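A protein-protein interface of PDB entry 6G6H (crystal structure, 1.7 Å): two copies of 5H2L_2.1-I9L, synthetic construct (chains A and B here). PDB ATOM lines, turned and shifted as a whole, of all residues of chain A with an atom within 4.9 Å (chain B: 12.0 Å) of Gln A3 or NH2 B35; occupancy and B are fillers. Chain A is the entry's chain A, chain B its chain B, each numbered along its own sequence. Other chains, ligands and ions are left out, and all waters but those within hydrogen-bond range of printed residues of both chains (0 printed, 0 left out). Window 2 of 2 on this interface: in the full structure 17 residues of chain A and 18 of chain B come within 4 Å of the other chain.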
ATOM      1  C   ACE A   1      26.911   8.130   4.491  1.00  0.00           C
ATOM      2  O   ACE A   1      26.332   8.673   3.546  1.00  0.00           O
ATOM      3  CH3 ACE A   1      27.424   8.942   5.637  1.00  0.00           C
ATOM      4  N   THR A   2      27.125   6.809   4.528  1.00  0.00           N
ATOM      5  CA  THR A   2      27.796   6.090   5.607  1.00  0.00           C
ATOM      6  C   THR A   2      28.862   5.139   5.063  1.00  0.00           C
ATOM      7  O   THR A   2      29.181   4.128   5.690  1.00  0.00           O
ATOM      8  CB  THR A   2      26.797   5.259   6.455  1.00  0.00           C
ATOM      9  OG1 THR A   2      26.181   4.257   5.637  1.00  0.00           O
ATOM     10  CG2 THR A   2      25.714   6.150   7.052  1.00  0.00           C
ATOM     11  N   GLN A   3      29.416   5.466   3.895  1.00  0.00           N
ATOM     12  CA  GLN A   3      30.310   4.526   3.222  1.00  0.00           C
ATOM     13  C   GLN A   3      31.607   4.314   4.003  1.00  0.00           C
ATOM     14  O   GLN A   3      32.105   3.181   4.091  1.00  0.00           O
ATOM     15  CB  GLN A   3      30.592   5.017   1.803  1.00  0.00           C
ATOM     16  CG  GLN A   3      29.356   4.975   0.904  1.00  0.00           C
ATOM     17  CD  GLN A   3      29.446   5.921  -0.280  1.00  0.00           C
ATOM     18  OE1 GLN A   3      29.598   7.131  -0.111  1.00  0.00           O
ATOM     19  NE2 GLN A   3      29.342   5.373  -1.486  1.00  0.00           N
ATOM     20  N   GLU A   4      32.173   5.385   4.576  1.00  0.00           N
ATOM     21  CA  GLU A   4      33.410   5.236   5.346  1.00  0.00           C
ATOM     22  C   GLU A   4      33.199   4.341   6.562  1.00  0.00           C
ATOM     23  O   GLU A   4      34.060   3.509   6.887  1.00  0.00           O
ATOM     24  CB  GLU A   4      33.947   6.613   5.771  1.00  0.00           C
ATOM     25  CG  GLU A   4      34.400   7.470   4.606  1.00  0.00           C
ATOM     26  CD  GLU A   4      34.875   8.854   5.022  1.00  0.00           C
ATOM     27  OE1 GLU A   4      34.944   9.129   6.242  1.00  0.00           O
ATOM     28  OE2 GLU A   4      35.179   9.666   4.121  1.00  0.00           O
ATOM     29  N   TYR A   5      32.051   4.483   7.235  1.00  0.00           N
ATOM     30  CA  TYR A   5      31.711   3.609   8.359  1.00  0.00           C
ATOM     31  C   TYR A   5      31.667   2.141   7.936  1.00  0.00           C
ATOM     32  O   TYR A   5      32.233   1.270   8.610  1.00  0.00           O
ATOM     33  CB  TYR A   5      30.364   4.027   8.951  1.00  0.00           C
ATOM     34  CG  TYR A   5      29.776   2.988   9.874  1.00  0.00           C
ATOM     35  CD1 TYR A   5      30.300   2.788  11.144  1.00  0.00           C
ATOM     36  CD2 TYR A   5      28.711   2.193   9.473  1.00  0.00           C
ATOM     37  CE1 TYR A   5      29.778   1.824  11.992  1.00  0.00           C
ATOM     38  CE2 TYR A   5      28.180   1.227  10.317  1.00  0.00           C
ATOM     39  CZ  TYR A   5      28.720   1.053  11.575  1.00  0.00           C
ATOM     40  OH  TYR A   5      28.201   0.101  12.420  1.00  0.00           O
ATOM     41  N   LEU A   6      30.973   1.850   6.831  1.00  0.00           N
ATOM     42  CA  LEU A   6      30.842   0.479   6.341  1.00  0.00           C
ATOM     43  C   LEU A   6      32.181  -0.114   5.912  1.00  0.00           C
ATOM     44  O   LEU A   6      32.409  -1.326   6.080  1.00  0.00           O
ATOM     45  CB  LEU A   6      29.835   0.448   5.175  1.00  0.00           C
ATOM     46  CG  LEU A   6      28.401   0.861   5.536  1.00  0.00           C
ATOM     47  CD1 LEU A   6      27.558   1.173   4.321  1.00  0.00           C
ATOM     48  CD2 LEU A   6      27.748  -0.282   6.275  1.00  0.00           C
ATOM     49  N   LEU A   7      33.073   0.698   5.336  1.00  0.00           N
ATOM     50  CA  LEU A   7      34.384   0.171   4.955  1.00  0.00           C
ATOM     51  C   LEU A   7      35.242  -0.110   6.188  1.00  0.00           C
ATOM     52  O   LEU A   7      36.007  -1.085   6.209  1.00  0.00           O
ATOM     53  CB  LEU A   7      35.090   1.142   4.002  1.00  0.00           C
ATOM     54  CG  LEU A   7      34.469   1.281   2.605  1.00  0.00           C
ATOM     55  CD1 LEU A   7      35.019   2.506   1.893  1.00  0.00           C
ATOM     56  CD2 LEU A   7      34.731   0.038   1.755  1.00  0.00           C
ATOM     57  N   GLN B  24      30.095  -9.771   6.661  1.00  0.00           N
ATOM     58  CA  GLN B  24      30.729  -9.042   5.563  1.00  0.00           C
ATOM     59  C   GLN B  24      29.757  -8.841   4.401  1.00  0.00           C
ATOM     60  O   GLN B  24      29.711  -7.761   3.805  1.00  0.00           O
ATOM     61  CB  GLN B  24      32.000  -9.784   5.110  1.00  0.00           C
ATOM     62  CG  GLN B  24      33.100  -9.783   6.185  1.00  0.00           C
ATOM     63  CD  GLN B  24      34.219 -10.784   5.892  1.00  0.00           C
ATOM     64  OE1 GLN B  24      34.665 -11.513   6.781  1.00  0.00           O
ATOM     65  NE2 GLN B  24      34.673 -10.814   4.646  1.00  0.00           N
ATOM     66  N   LYS B  26      26.561  -8.507   4.600  1.00  0.00           N
ATOM     67  CA  LYS B  26      25.572  -7.492   4.951  1.00  0.00           C
ATOM     68  C   LYS B  26      26.144  -6.091   4.770  1.00  0.00           C
ATOM     69  O   LYS B  26      25.428  -5.174   4.345  1.00  0.00           O
ATOM     70  CB  LYS B  26      25.066  -7.704   6.386  1.00  0.00           C
ATOM     71  CG  LYS B  26      24.089  -8.889   6.582  1.00  0.00           C
ATOM     72  N   MET B  27      27.437  -5.908   5.068  1.00  0.00           N
ATOM     73  CA  MET B  27      28.061  -4.601   4.878  1.00  0.00           C
ATOM     74  C   MET B  27      28.156  -4.247   3.396  1.00  0.00           C
ATOM     75  O   MET B  27      27.901  -3.102   3.013  1.00  0.00           O
ATOM     76  CB  MET B  27      29.450  -4.571   5.525  1.00  0.00           C
ATOM     77  CG  MET B  27      29.455  -4.828   7.027  1.00  0.00           C
ATOM     78  SD  MET B  27      28.520  -3.607   7.970  1.00  0.00           S
ATOM     79  CE  MET B  27      27.966  -4.620   9.341  1.00  0.00           C
ATOM     80  N   LEU B  28      28.526  -5.217   2.550  1.00  0.00           N
ATOM     81  CA  LEU B  28      28.559  -4.983   1.105  1.00  0.00           C
ATOM     82  C   LEU B  28      27.178  -4.635   0.555  1.00  0.00           C
ATOM     83  O   LEU B  28      27.056  -3.817  -0.365  1.00  0.00           O
ATOM     84  CB  LEU B  28      29.112  -6.226   0.395  1.00  0.00           C
ATOM     85  CG  LEU B  28      30.586  -6.516   0.642  1.00  0.00           C
ATOM     86  CD1 LEU B  28      30.945  -7.900   0.090  1.00  0.00           C
ATOM     87  CD2 LEU B  28      31.434  -5.440  -0.020  1.00  0.00           C
ATOM     88  N   LYS B  29      26.131  -5.279   1.074  1.00  0.00           N
ATOM     89  CA  LYS B  29      24.776  -4.985   0.622  1.00  0.00           C
ATOM     90  C   LYS B  29      24.412  -3.534   0.903  1.00  0.00           C
ATOM     91  O   LYS B  29      23.790  -2.867   0.066  1.00  0.00           O
ATOM     92  CB  LYS B  29      23.789  -5.931   1.304  1.00  0.00           C
ATOM     93  N   GLU B  30      24.826  -3.014   2.061  1.00  0.00           N
ATOM     94  CA  GLU B  30      24.533  -1.624   2.382  1.00  0.00           C
ATOM     95  C   GLU B  30      25.342  -0.664   1.517  1.00  0.00           C
ATOM     96  O   GLU B  30      24.829   0.384   1.107  1.00  0.00           O
ATOM     97  CB  GLU B  30      24.779  -1.361   3.867  1.00  0.00           C
ATOM     98  CG  GLU B  30      23.908  -2.195   4.789  1.00  0.00           C
ATOM     99  CD  GLU B  30      23.539  -1.462   6.064  1.00  0.00           C
ATOM    100  OE1 GLU B  30      23.072  -0.305   5.972  1.00  0.00           O
ATOM    101  OE2 GLU B  30      23.722  -2.040   7.158  1.00  0.00           O
ATOM    102  N   LEU B  31      26.603  -0.998   1.223  1.00  0.00           N
ATOM    103  CA  LEU B  31      27.396  -0.157   0.327  1.00  0.00           C
ATOM    104  C   LEU B  31      26.768  -0.085  -1.059  1.00  0.00           C
ATOM    105  O   LEU B  31      26.749   0.980  -1.691  1.00  0.00           O
ATOM    106  CB  LEU B  31      28.824  -0.697   0.223  1.00  0.00           C
ATOM    107  CG  LEU B  31      29.735  -0.441   1.417  1.00  0.00           C
ATOM    108  CD1 LEU B  31      31.020  -1.233   1.255  1.00  0.00           C
ATOM    109  CD2 LEU B  31      30.036   1.048   1.517  1.00  0.00           C
ATOM    110  N   GLU B  32      26.241  -1.208  -1.542  1.00  0.00           N
ATOM    111  CA  GLU B  32      25.682  -1.257  -2.891  1.00  0.00           C
ATOM    112  C   GLU B  32      24.522  -0.281  -3.058  1.00  0.00           C
ATOM    113  O   GLU B  32      24.356   0.304  -4.134  1.00  0.00           O
ATOM    114  CB  GLU B  32      25.253  -2.692  -3.212  1.00  0.00           C
ATOM    115  CG  GLU B  32      24.974  -2.964  -4.691  1.00  0.00           C
ATOM    116  CD  GLU B  32      23.583  -2.528  -5.110  1.00  0.00           C
ATOM    117  OE1 GLU B  32      22.719  -2.385  -4.220  1.00  0.00           O
ATOM    118  OE2 GLU B  32      23.358  -2.326  -6.323  1.00  0.00           O
ATOM    119  N   LYS B  33      23.722  -0.078  -2.010  1.00  0.00           N
ATOM    120  CA  LYS B  33      22.616   0.873  -2.080  1.00  0.00           C
ATOM    121  C   LYS B  33      23.061   2.333  -2.117  1.00  0.00           C
ATOM    122  O   LYS B  33      22.220   3.207  -2.349  1.00  0.00           O
ATOM    123  CB  LYS B  33      21.679   0.668  -0.890  1.00  0.00           C
ATOM    124  CG  LYS B  33      21.107  -0.722  -0.777  1.00  0.00           C
ATOM    125  CD  LYS B  33      20.188  -0.824   0.423  1.00  0.00           C
ATOM    126  CE  LYS B  33      19.728  -2.247   0.637  1.00  0.00           C
ATOM    127  NZ  LYS B  33      19.160  -2.825  -0.606  1.00  0.00           N
ATOM    128  N   GLN B  34      24.337   2.628  -1.889  1.00  0.00           N
ATOM    129  CA  GLN B  34      24.797   4.016  -1.881  1.00  0.00           C
ATOM    130  C   GLN B  34      25.659   4.341  -3.103  1.00  0.00           C
ATOM    131  O   GLN B  34      25.905   3.472  -3.942  1.00  0.00           O
ATOM    132  CB  GLN B  34      25.574   4.309  -0.593  1.00  0.00           C
ATOM    133  CG  GLN B  34      24.945   3.689   0.645  1.00  0.00           C
ATOM    134  CD  GLN B  34      25.350   4.372   1.943  1.00  0.00           C
ATOM    135  OE1 GLN B  34      25.913   5.471   1.944  1.00  0.00           O
ATOM    136  NE2 GLN B  34      25.078   3.710   3.060  1.00  0.00           N
ATOM    137  N   NH2 B  35      26.199   5.572  -3.236  1.00  0.00           N
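Of the 11 printed residues of chain B, 5 touch a printed residue of chain A. Hydrophobic or aromatic side chains of chain B within 4 Å of the printed part of chain A: Met B27 and Leu B31. Among the printed residues, no Asp or Glu carboxylate lies within 4 Å of a Lys or Arg side-chain nitrogen of the other chain.
Among the printed residues, pairs that only touch across the chains: ACE A1 with Gln B34, Gln A3 with Leu B31, Gln A3 with Gln B34, Gln A3 with NH2 B35, Leu A6 with Met B27, Leu A6 with Glu B30, Leu A6 with Leu B31, Leu A6 with Gln B34 and Leu A7 with Leu B31.
No position is printed for both chains. Of the 10 pairs that touch across the chains among the printed residues, none has its exchanged pair printed and touching as well.
Gln A3 touches three residues of chain B. Of chain A, only Gln A3 comes within 4 Å of NH2 B35. Of chain B, only Gln B34 (3.6 Å) comes within 4 Å of ACE A1. Thr A2 touches just one residue of chain B: Gln B34. No residue of chain B comes within 4 Å of Glu A4. Of the printed residues of chain B, Leu A7 touches Leu B31. Printed residues of chain A within 4 Å of Leu B31: Gln A3, Leu A6 and Leu A7. Printed residues of chain A within 4 Å of Met B27: Leu A6. Of the printed residues of chain A, Gln B34 touches ACE A1 (3.6 Å), Thr A2 (2.9 Å), Gln A3 (3.6 Å) and Leu A6 (3.8 Å). Printed residues of chain A within 4 Å of Glu B30: Leu A6 (3.8 Å). The nearest residue of chain B that does not touch Gln A3 is Glu B30 (6.5 Å).
NE2 of Gln B34 lies within hydrogen-bond range of OG1 of Thr A2.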
